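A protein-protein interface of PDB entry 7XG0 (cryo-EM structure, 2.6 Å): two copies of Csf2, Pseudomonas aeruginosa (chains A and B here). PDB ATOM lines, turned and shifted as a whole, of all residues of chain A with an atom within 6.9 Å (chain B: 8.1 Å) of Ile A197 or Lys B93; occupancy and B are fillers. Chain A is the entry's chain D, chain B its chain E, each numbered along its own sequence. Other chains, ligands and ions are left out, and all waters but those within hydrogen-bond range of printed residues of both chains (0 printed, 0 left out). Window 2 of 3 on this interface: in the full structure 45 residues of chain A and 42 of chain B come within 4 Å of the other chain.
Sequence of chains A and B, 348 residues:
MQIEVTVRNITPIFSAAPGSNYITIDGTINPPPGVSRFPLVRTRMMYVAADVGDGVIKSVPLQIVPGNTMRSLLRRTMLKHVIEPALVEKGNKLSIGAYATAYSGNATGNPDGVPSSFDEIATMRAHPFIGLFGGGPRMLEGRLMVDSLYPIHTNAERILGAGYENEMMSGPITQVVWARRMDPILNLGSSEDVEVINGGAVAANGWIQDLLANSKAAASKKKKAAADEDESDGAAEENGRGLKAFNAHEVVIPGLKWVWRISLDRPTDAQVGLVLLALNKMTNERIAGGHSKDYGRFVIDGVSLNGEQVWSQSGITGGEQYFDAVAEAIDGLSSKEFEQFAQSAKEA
The backbone carbonyl oxygen of Glu A195 is in hydrogen-bond range of the side-chain amino group of Lys B93. The backbone NH of Leu B94 lies within hydrogen-bond range of the backbone carbonyl oxygen of Val A196 (2.7 Å). ND2 of Asn A198 sits at hydrogen-bond distance from O of Lys B93, at 3.3 Å. N of Asn A198 sits at hydrogen-bond distance from O of Leu B94, at 2.5 Å.
OE2 of Glu B84 lies within hydrogen-bond range of OH of Tyr B103 (2.7 Å). The backbone carbonyl oxygen (O) of Leu B87 lies within hydrogen-bond range of the backbone NH (N) of Asn B92 (2.7 Å).
Among the printed residues, merely in contact across the chains: Leu A188 with Tyr B99, Ile A197 with Leu B94, Val A196 with Lys B93, Glu A195 with Val B88, Ile A197 with Tyr B99, Val A196 with Tyr B99, Asp A193 with Tyr B99, Ile A197 with Lys B93, Ile A185 with Tyr B99, Ile A185 with Ile B96, Val A196 with Leu B87, Ala A203 with Ile B96, Ile A197 with Ile B96, Val A196 with Val B88, Val A196 with Glu B84 and Ala A204 with Ile B96.
Of the printed residues of chain B, Asp A193 touches Tyr B99. Of the printed residues of chain B, Val A196 touches Glu B84, Leu B87, Val B88, Lys B93, Leu B94 and Tyr B99. Of the printed residues of chain A, Leu B87 touches Val A196 (3.7 Å). Of chain A, only Glu A195, Val A196, Ile A197 and Asn A198 come within 4 Å of Lys B93. Glu B339 touches none of the printed residues of chain A.
Of the 21 printed residues of chain B, 7 touch a printed residue of chain A. Among the printed residues, 20 pairs touch across the chains. Among the printed residues, no Asp or Glu carboxylate lies within 4 Å of a Lys or Arg side-chain nitrogen of the other chain.
No position is printed for both chains. Of the 20 pairs that touch across the chains among the printed residues, none has its exchanged pair printed and touching as well.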
ATOM      1  N   ILE A 185      29.471   7.079 -37.625  1.00  0.00           N
ATOM      2  CA  ILE A 185      30.470   7.041 -36.560  1.00  0.00           C
ATOM      3  C   ILE A 185      31.865   7.236 -37.144  1.00  0.00           C
ATOM      4  O   ILE A 185      32.772   7.749 -36.476  1.00  0.00           O
ATOM      5  CB  ILE A 185      30.342   5.724 -35.768  1.00  0.00           C
ATOM      6  CG1 ILE A 185      28.876   5.433 -35.407  1.00  0.00           C
ATOM      7  CG2 ILE A 185      31.158   5.763 -34.480  1.00  0.00           C
ATOM      8  CD1 ILE A 185      28.130   6.556 -34.678  1.00  0.00           C
ATOM      9  N   LEU A 188      32.559  10.970 -37.335  1.00  0.00           N
ATOM     10  CA  LEU A 188      32.888  11.659 -36.093  1.00  0.00           C
ATOM     11  C   LEU A 188      34.319  12.173 -36.137  1.00  0.00           C
ATOM     12  O   LEU A 188      35.230  11.467 -36.576  1.00  0.00           O
ATOM     13  CB  LEU A 188      32.704  10.718 -34.899  1.00  0.00           C
ATOM     14  CG  LEU A 188      31.281  10.457 -34.410  1.00  0.00           C
ATOM     15  CD1 LEU A 188      31.265   9.347 -33.377  1.00  0.00           C
ATOM     16  CD2 LEU A 188      30.718  11.727 -33.819  1.00  0.00           C
ATOM     17  N   ASP A 193      31.893  16.637 -31.538  1.00  0.00           N
ATOM     18  CA  ASP A 193      30.986  15.874 -32.387  1.00  0.00           C
ATOM     19  C   ASP A 193      30.343  14.718 -31.630  1.00  0.00           C
ATOM     20  O   ASP A 193      29.299  14.208 -32.051  1.00  0.00           O
ATOM     21  CB  ASP A 193      31.741  15.346 -33.608  1.00  0.00           C
ATOM     22  CG  ASP A 193      31.686  16.299 -34.785  1.00  0.00           C
ATOM     23  OD1 ASP A 193      31.559  17.521 -34.561  1.00  0.00           O
ATOM     24  OD2 ASP A 193      31.776  15.825 -35.938  1.00  0.00           O
ATOM     25  N   VAL A 194      30.943  14.298 -30.516  1.00  0.00           N
ATOM     26  CA  VAL A 194      30.590  13.063 -29.833  1.00  0.00           C
ATOM     27  C   VAL A 194      29.875  13.318 -28.507  1.00  0.00           C
ATOM     28  O   VAL A 194      29.386  12.375 -27.878  1.00  0.00           O
ATOM     29  CB  VAL A 194      31.843  12.182 -29.637  1.00  0.00           C
ATOM     30  CG1 VAL A 194      32.587  12.513 -28.335  1.00  0.00           C
ATOM     31  CG2 VAL A 194      31.507  10.700 -29.744  1.00  0.00           C
ATOM     32  N   GLU A 195      29.761  14.586 -28.095  1.00  0.00           N
ATOM     33  CA  GLU A 195      29.166  14.935 -26.806  1.00  0.00           C
ATOM     34  C   GLU A 195      27.675  14.618 -26.739  1.00  0.00           C
ATOM     35  O   GLU A 195      27.142  14.419 -25.641  1.00  0.00           O
ATOM     36  CB  GLU A 195      29.409  16.422 -26.524  1.00  0.00           C
ATOM     37  CG  GLU A 195      29.226  16.846 -25.072  1.00  0.00           C
ATOM     38  CD  GLU A 195      29.226  18.353 -24.899  1.00  0.00           C
ATOM     39  OE1 GLU A 195      28.131  18.950 -24.884  1.00  0.00           O
ATOM     40  OE2 GLU A 195      30.323  18.938 -24.778  1.00  0.00           O
ATOM     41  N   VAL A 196      26.997  14.529 -27.885  1.00  0.00           N
ATOM     42  CA  VAL A 196      25.576  14.195 -27.892  1.00  0.00           C
ATOM     43  C   VAL A 196      25.368  12.684 -27.782  1.00  0.00           C
ATOM     44  O   VAL A 196      24.239  12.216 -27.589  1.00  0.00           O
ATOM     45  CB  VAL A 196      24.920  14.790 -29.155  1.00  0.00           C
ATOM     46  CG1 VAL A 196      25.130  13.886 -30.352  1.00  0.00           C
ATOM     47  CG2 VAL A 196      23.441  15.076 -28.929  1.00  0.00           C
ATOM     48  N   ILE A 197      26.437  11.898 -27.877  1.00  0.00           N
ATOM     49  CA  ILE A 197      26.351  10.444 -27.798  1.00  0.00           C
ATOM     50  C   ILE A 197      26.550  10.006 -26.353  1.00  0.00           C
ATOM     51  O   ILE A 197      27.475  10.464 -25.673  1.00  0.00           O
ATOM     52  CB  ILE A 197      27.384   9.785 -28.733  1.00  0.00           C
ATOM     53  CG1 ILE A 197      27.118  10.189 -30.181  1.00  0.00           C
ATOM     54  CG2 ILE A 197      27.356   8.269 -28.611  1.00  0.00           C
ATOM     55  CD1 ILE A 197      28.192   9.756 -31.144  1.00  0.00           C
ATOM     56  N   ASN A 198      25.653   9.139 -25.873  1.00  0.00           N
ATOM     57  CA  ASN A 198      25.822   8.516 -24.565  1.00  0.00           C
ATOM     58  C   ASN A 198      27.062   7.633 -24.557  1.00  0.00           C
ATOM     59  O   ASN A 198      27.211   6.740 -25.396  1.00  0.00           O
ATOM     60  CB  ASN A 198      24.585   7.692 -24.204  1.00  0.00           C
ATOM     61  CG  ASN A 198      24.103   7.951 -22.793  1.00  0.00           C
ATOM     62  OD1 ASN A 198      24.767   7.593 -21.821  1.00  0.00           O
ATOM     63  ND2 ASN A 198      22.936   8.575 -22.672  1.00  0.00           N
ATOM     64  N   GLY A 199      27.955   7.887 -23.604  1.00  0.00           N
ATOM     65  CA  GLY A 199      29.261   7.270 -23.588  1.00  0.00           C
ATOM     66  C   GLY A 199      30.327   8.043 -24.332  1.00  0.00           C
ATOM     67  O   GLY A 199      31.468   8.108 -23.856  1.00  0.00           O
ATOM     68  N   GLY A 200      29.989   8.637 -25.472  1.00  0.00           N
ATOM     69  CA  GLY A 200      30.931   9.491 -26.174  1.00  0.00           C
ATOM     70  C   GLY A 200      32.009   8.698 -26.880  1.00  0.00           C
ATOM     71  O   GLY A 200      31.733   7.896 -27.785  1.00  0.00           O
ATOM     72  N   ALA A 201      33.257   8.937 -26.466  1.00  0.00           N
ATOM     73  CA  ALA A 201      34.405   8.310 -27.114  1.00  0.00           C
ATOM     74  C   ALA A 201      34.437   6.807 -26.878  1.00  0.00           C
ATOM     75  O   ALA A 201      34.886   6.059 -27.752  1.00  0.00           O
ATOM     76  CB  ALA A 201      35.700   8.953 -26.621  1.00  0.00           C
ATOM     77  N   ALA A 203      31.733   4.757 -26.513  1.00  0.00           N
ATOM     78  CA  ALA A 203      30.741   4.160 -27.404  1.00  0.00           C
ATOM     79  C   ALA A 203      31.179   4.240 -28.862  1.00  0.00           C
ATOM     80  O   ALA A 203      30.948   3.304 -29.641  1.00  0.00           O
ATOM     81  CB  ALA A 203      29.388   4.846 -27.213  1.00  0.00           C
ATOM     82  N   ALA A 204      31.828   5.348 -29.241  1.00  0.00           N
ATOM     83  CA  ALA A 204      32.346   5.487 -30.600  1.00  0.00           C
ATOM     84  C   ALA A 204      33.432   4.455 -30.889  1.00  0.00           C
ATOM     85  O   ALA A 204      33.403   3.791 -31.932  1.00  0.00           O
ATOM     86  CB  ALA A 204      32.874   6.906 -30.811  1.00  0.00           C
ATOM     87  N   GLU B  84      21.709  19.040 -32.254  1.00  0.00           N
ATOM     88  CA  GLU B  84      22.726  18.764 -31.234  1.00  0.00           C
ATOM     89  C   GLU B  84      22.938  19.894 -30.225  1.00  0.00           C
ATOM     90  O   GLU B  84      23.141  19.579 -29.041  1.00  0.00           O
ATOM     91  CB  GLU B  84      24.051  18.357 -31.886  1.00  0.00           C
ATOM     92  CG  GLU B  84      24.102  16.947 -32.424  1.00  0.00           C
ATOM     93  CD  GLU B  84      25.353  16.702 -33.239  1.00  0.00           C
ATOM     94  OE1 GLU B  84      26.434  17.175 -32.825  1.00  0.00           O
ATOM     95  OE2 GLU B  84      25.259  16.048 -34.294  1.00  0.00           O
ATOM     96  N   LEU B  87      20.145  19.518 -27.863  1.00  0.00           N
ATOM     97  CA  LEU B  87      20.210  18.301 -27.060  1.00  0.00           C
ATOM     98  C   LEU B  87      21.270  18.409 -25.967  1.00  0.00           C
ATOM     99  O   LEU B  87      21.026  18.026 -24.817  1.00  0.00           O
ATOM    100  CB  LEU B  87      20.478  17.095 -27.959  1.00  0.00           C
ATOM    101  CG  LEU B  87      19.297  16.588 -28.791  1.00  0.00           C
ATOM    102  CD1 LEU B  87      19.741  15.479 -29.725  1.00  0.00           C
ATOM    103  CD2 LEU B  87      18.159  16.120 -27.900  1.00  0.00           C
ATOM    104  N   VAL B  88      22.455  18.929 -26.301  1.00  0.00           N
ATOM    105  CA  VAL B  88      23.513  19.029 -25.297  1.00  0.00           C
ATOM    106  C   VAL B  88      23.312  20.265 -24.429  1.00  0.00           C
ATOM    107  O   VAL B  88      23.915  20.389 -23.357  1.00  0.00           O
ATOM    108  CB  VAL B  88      24.907  19.019 -25.955  1.00  0.00           C
ATOM    109  CG1 VAL B  88      25.041  17.853 -26.922  1.00  0.00           C
ATOM    110  CG2 VAL B  88      25.220  20.352 -26.629  1.00  0.00           C
ATOM    111  N   LYS B  90      20.264  21.034 -23.173  1.00  0.00           N
ATOM    112  CA  LYS B  90      19.359  20.509 -22.161  1.00  0.00           C
ATOM    113  C   LYS B  90      19.906  19.270 -21.466  1.00  0.00           C
ATOM    114  O   LYS B  90      19.221  18.707 -20.606  1.00  0.00           O
ATOM    115  CB  LYS B  90      18.001  20.188 -22.790  1.00  0.00           C
ATOM    116  CG  LYS B  90      17.007  21.330 -22.715  1.00  0.00           C
ATOM    117  CD  LYS B  90      15.924  21.188 -23.770  1.00  0.00           C
ATOM    118  CE  LYS B  90      15.076  22.447 -23.873  1.00  0.00           C
ATOM    119  NZ  LYS B  90      15.676  23.611 -23.164  1.00  0.00           N
ATOM    120  N   GLY B  91      21.114  18.833 -21.815  1.00  0.00           N
ATOM    121  CA  GLY B  91      21.714  17.666 -21.205  1.00  0.00           C
ATOM    122  C   GLY B  91      21.286  16.336 -21.784  1.00  0.00           C
ATOM    123  O   GLY B  91      21.730  15.294 -21.285  1.00  0.00           O
ATOM    124  N   ASN B  92      20.440  16.333 -22.811  1.00  0.00           N
ATOM    125  CA  ASN B  92      20.004  15.083 -23.417  1.00  0.00           C
ATOM    126  C   ASN B  92      21.123  14.474 -24.251  1.00  0.00           C
ATOM    127  O   ASN B  92      21.778  15.161 -25.041  1.00  0.00           O
ATOM    128  CB  ASN B  92      18.770  15.318 -24.287  1.00  0.00           C
ATOM    129  CG  ASN B  92      17.578  15.803 -23.489  1.00  0.00           C
ATOM    130  OD1 ASN B  92      17.105  16.923 -23.678  1.00  0.00           O
ATOM    131  ND2 ASN B  92      17.085  14.959 -22.590  1.00  0.00           N
ATOM    132  N   LYS B  93      21.340  13.173 -24.073  1.00  0.00           N
ATOM    133  CA  LYS B  93      22.396  12.456 -24.782  1.00  0.00           C
ATOM    134  C   LYS B  93      21.774  11.253 -25.474  1.00  0.00           C
ATOM    135  O   LYS B  93      21.207  10.376 -24.814  1.00  0.00           O
ATOM    136  CB  LYS B  93      23.510  12.022 -23.829  1.00  0.00           C
ATOM    137  CG  LYS B  93      24.399  13.158 -23.354  1.00  0.00           C
ATOM    138  CD  LYS B  93      25.369  12.688 -22.282  1.00  0.00           C
ATOM    139  CE  LYS B  93      26.792  12.626 -22.811  1.00  0.00           C
ATOM    140  NZ  LYS B  93      27.283  13.963 -23.244  1.00  0.00           N
ATOM    141  N   LEU B  94      21.877  11.215 -26.800  1.00  0.00           N
ATOM    142  CA  LEU B  94      21.380  10.083 -27.563  1.00  0.00           C
ATOM    143  C   LEU B  94      22.293   8.875 -27.389  1.00  0.00           C
ATOM    144  O   LEU B  94      23.463   8.993 -27.021  1.00  0.00           O
ATOM    145  CB  LEU B  94      21.284  10.432 -29.048  1.00  0.00           C
ATOM    146  CG  LEU B  94      20.694  11.785 -29.436  1.00  0.00           C
ATOM    147  CD1 LEU B  94      20.838  12.013 -30.930  1.00  0.00           C
ATOM    148  CD2 LEU B  94      19.241  11.843 -29.028  1.00  0.00           C
ATOM    149  N   SER B  95      21.742   7.698 -27.667  1.00  0.00           N
ATOM    150  CA  SER B  95      22.571   6.510 -27.770  1.00  0.00           C
ATOM    151  C   SER B  95      23.365   6.540 -29.072  1.00  0.00           C
ATOM    152  O   SER B  95      23.128   7.368 -29.958  1.00  0.00           O
ATOM    153  CB  SER B  95      21.718   5.242 -27.702  1.00  0.00           C
ATOM    154  OG  SER B  95      22.520   4.080 -27.837  1.00  0.00           O
ATOM    155  N   ILE B  96      24.336   5.629 -29.172  1.00  0.00           N
ATOM    156  CA  ILE B  96      25.145   5.536 -30.384  1.00  0.00           C
ATOM    157  C   ILE B  96      24.291   5.048 -31.555  1.00  0.00           C
ATOM    158  O   ILE B  96      24.448   5.507 -32.696  1.00  0.00           O
ATOM    159  CB  ILE B  96      26.388   4.652 -30.122  1.00  0.00           C
ATOM    160  CG1 ILE B  96      27.362   4.686 -31.301  1.00  0.00           C
ATOM    161  CG2 ILE B  96      26.033   3.220 -29.686  1.00  0.00           C
ATOM    162  CD1 ILE B  96      28.481   5.681 -31.109  1.00  0.00           C
ATOM    163  N   GLY B  97      23.331   4.160 -31.274  1.00  0.00           N
ATOM    164  CA  GLY B  97      22.369   3.766 -32.288  1.00  0.00           C
ATOM    165  C   GLY B  97      21.417   4.887 -32.655  1.00  0.00           C
ATOM    166  O   GLY B  97      21.031   5.028 -33.816  1.00  0.00           O
ATOM    167  N   ALA B  98      21.029   5.704 -31.670  1.00  0.00           N
ATOM    168  CA  ALA B  98      20.189   6.863 -31.950  1.00  0.00           C
ATOM    169  C   ALA B  98      20.936   7.918 -32.756  1.00  0.00           C
ATOM    170  O   ALA B  98      20.339   8.569 -33.621  1.00  0.00           O
ATOM    171  CB  ALA B  98      19.662   7.460 -30.646  1.00  0.00           C
ATOM    172  N   TYR B  99      22.236   8.082 -32.500  1.00  0.00           N
ATOM    173  CA  TYR B  99      23.056   8.987 -33.301  1.00  0.00           C
ATOM    174  C   TYR B  99      23.177   8.485 -34.736  1.00  0.00           C
ATOM    175  O   TYR B  99      23.105   9.271 -35.693  1.00  0.00           O
ATOM    176  CB  TYR B  99      24.434   9.128 -32.653  1.00  0.00           C
ATOM    177  CG  TYR B  99      25.361  10.117 -33.322  1.00  0.00           C
ATOM    178  CD1 TYR B  99      25.308  11.461 -32.991  1.00  0.00           C
ATOM    179  CD2 TYR B  99      26.306   9.707 -34.260  1.00  0.00           C
ATOM    180  CE1 TYR B  99      26.156  12.374 -33.570  1.00  0.00           C
ATOM    181  CE2 TYR B  99      27.157  10.619 -34.858  1.00  0.00           C
ATOM    182  CZ  TYR B  99      27.076  11.952 -34.505  1.00  0.00           C
ATOM    183  OH  TYR B  99      27.910  12.877 -35.089  1.00  0.00           O
ATOM    184  N   ALA B 100      23.367   7.169 -34.899  1.00  0.00           N
ATOM    185  CA  ALA B 100      23.440   6.582 -36.233  1.00  0.00           C
ATOM    186  C   ALA B 100      22.106   6.684 -36.964  1.00  0.00           C
ATOM    187  O   ALA B 100      22.070   6.872 -38.183  1.00  0.00           O
ATOM    188  CB  ALA B 100      23.889   5.124 -36.137  1.00  0.00           C
ATOM    189  N   TYR B 103      21.906  10.439 -38.134  1.00  0.00           N
ATOM    190  CA  TYR B 103      22.732  10.890 -39.255  1.00  0.00           C
ATOM    191  C   TYR B 103      22.561  10.002 -40.485  1.00  0.00           C
ATOM    192  O   TYR B 103      22.551  10.495 -41.616  1.00  0.00           O
ATOM    193  CB  TYR B 103      24.202  10.948 -38.848  1.00  0.00           C
ATOM    194  CG  TYR B 103      24.665  12.286 -38.332  1.00  0.00           C
ATOM    195  CD1 TYR B 103      25.152  13.257 -39.198  1.00  0.00           C
ATOM    196  CD2 TYR B 103      24.655  12.566 -36.975  1.00  0.00           C
ATOM    197  CE1 TYR B 103      25.584  14.484 -38.725  1.00  0.00           C
ATOM    198  CE2 TYR B 103      25.072  13.794 -36.502  1.00  0.00           C
ATOM    199  CZ  TYR B 103      25.543  14.744 -37.376  1.00  0.00           C
ATOM    200  OH  TYR B 103      25.972  15.961 -36.898  1.00  0.00           O
ATOM    201  N   LEU B 333      12.896  19.504 -26.829  1.00  0.00           N
ATOM    202  CA  LEU B 333      13.378  18.415 -27.670  1.00  0.00           C
ATOM    203  C   LEU B 333      14.101  17.384 -26.815  1.00  0.00           C
ATOM    204  O   LEU B 333      15.146  17.672 -26.223  1.00  0.00           O
ATOM    205  CB  LEU B 333      14.309  18.956 -28.754  1.00  0.00           C
ATOM    206  CG  LEU B 333      14.892  17.955 -29.750  1.00  0.00           C
ATOM    207  CD1 LEU B 333      13.787  17.368 -30.602  1.00  0.00           C
ATOM    208  CD2 LEU B 333      15.947  18.619 -30.620  1.00  0.00           C
ATOM    209  N   SER B 334      13.547  16.178 -26.760  1.00  0.00           N
ATOM    210  CA  SER B 334      14.025  15.147 -25.854  1.00  0.00           C
ATOM    211  C   SER B 334      14.736  14.056 -26.637  1.00  0.00           C
ATOM    212  O   SER B 334      14.485  13.853 -27.829  1.00  0.00           O
ATOM    213  CB  SER B 334      12.874  14.536 -25.040  1.00  0.00           C
ATOM    214  OG  SER B 334      12.040  13.735 -25.857  1.00  0.00           O
ATOM    215  N   SER B 335      15.640  13.360 -25.947  1.00  0.00           N
ATOM    216  CA  SER B 335      16.368  12.258 -26.558  1.00  0.00           C
ATOM    217  C   SER B 335      15.504  11.019 -26.741  1.00  0.00           C
ATOM    218  O   SER B 335      15.829  10.177 -27.586  1.00  0.00           O
ATOM    219  CB  SER B 335      17.593  11.911 -25.708  1.00  0.00           C
ATOM    220  OG  SER B 335      17.214  11.248 -24.516  1.00  0.00           O
ATOM    221  N   LYS B 336      14.407  10.900 -25.984  1.00  0.00           N
ATOM    222  CA  LYS B 336      13.655   9.649 -25.939  1.00  0.00           C
ATOM    223  C   LYS B 336      12.894   9.393 -27.237  1.00  0.00           C
ATOM    224  O   LYS B 336      12.647   8.233 -27.589  1.00  0.00           O
ATOM    225  CB  LYS B 336      12.718   9.645 -24.723  1.00  0.00           C
ATOM    226  CG  LYS B 336      11.364  10.314 -24.921  1.00  0.00           C
ATOM    227  CD  LYS B 336      10.217   9.392 -24.546  1.00  0.00           C
ATOM    228  CE  LYS B 336       8.931  10.177 -24.349  1.00  0.00           C
ATOM    229  NZ  LYS B 336       7.872   9.365 -23.691  1.00  0.00           N
ATOM    230  N   PHE B 338      14.182  10.092 -30.246  1.00  0.00           N
ATOM    231  CA  PHE B 338      15.222   9.478 -31.064  1.00  0.00           C
ATOM    232  C   PHE B 338      15.525   8.060 -30.595  1.00  0.00           C
ATOM    233  O   PHE B 338      15.828   7.181 -31.412  1.00  0.00           O
ATOM    234  CB  PHE B 338      16.491  10.328 -31.018  1.00  0.00           C
ATOM    235  CG  PHE B 338      16.352  11.669 -31.679  1.00  0.00           C
ATOM    236  CD1 PHE B 338      16.603  11.819 -33.033  1.00  0.00           C
ATOM    237  CD2 PHE B 338      15.981  12.783 -30.939  1.00  0.00           C
ATOM    238  CE1 PHE B 338      16.480  13.055 -33.640  1.00  0.00           C
ATOM    239  CE2 PHE B 338      15.855  14.023 -31.541  1.00  0.00           C
ATOM    240  CZ  PHE B 338      16.105  14.157 -32.894  1.00  0.00           C
ATOM    241  N   GLU B 339      15.451   7.824 -29.278  1.00  0.00           N
ATOM    242  CA  GLU B 339      15.728   6.496 -28.734  1.00  0.00           C
ATOM    243  C   GLU B 339      14.681   5.476 -29.168  1.00  0.00           C
ATOM    244  O   GLU B 339      15.029   4.357 -29.562  1.00  0.00           O
ATOM    245  CB  GLU B 339      15.807   6.548 -27.208  1.00  0.00           C
ATOM    246  CG  GLU B 339      17.011   7.295 -26.658  1.00  0.00           C
ATOM    247  CD  GLU B 339      18.334   6.672 -27.053  1.00  0.00           C
ATOM    248  OE1 GLU B 339      18.418   5.427 -27.139  1.00  0.00           O
ATOM    249  OE2 GLU B 339      19.293   7.436 -27.284  1.00  0.00           O
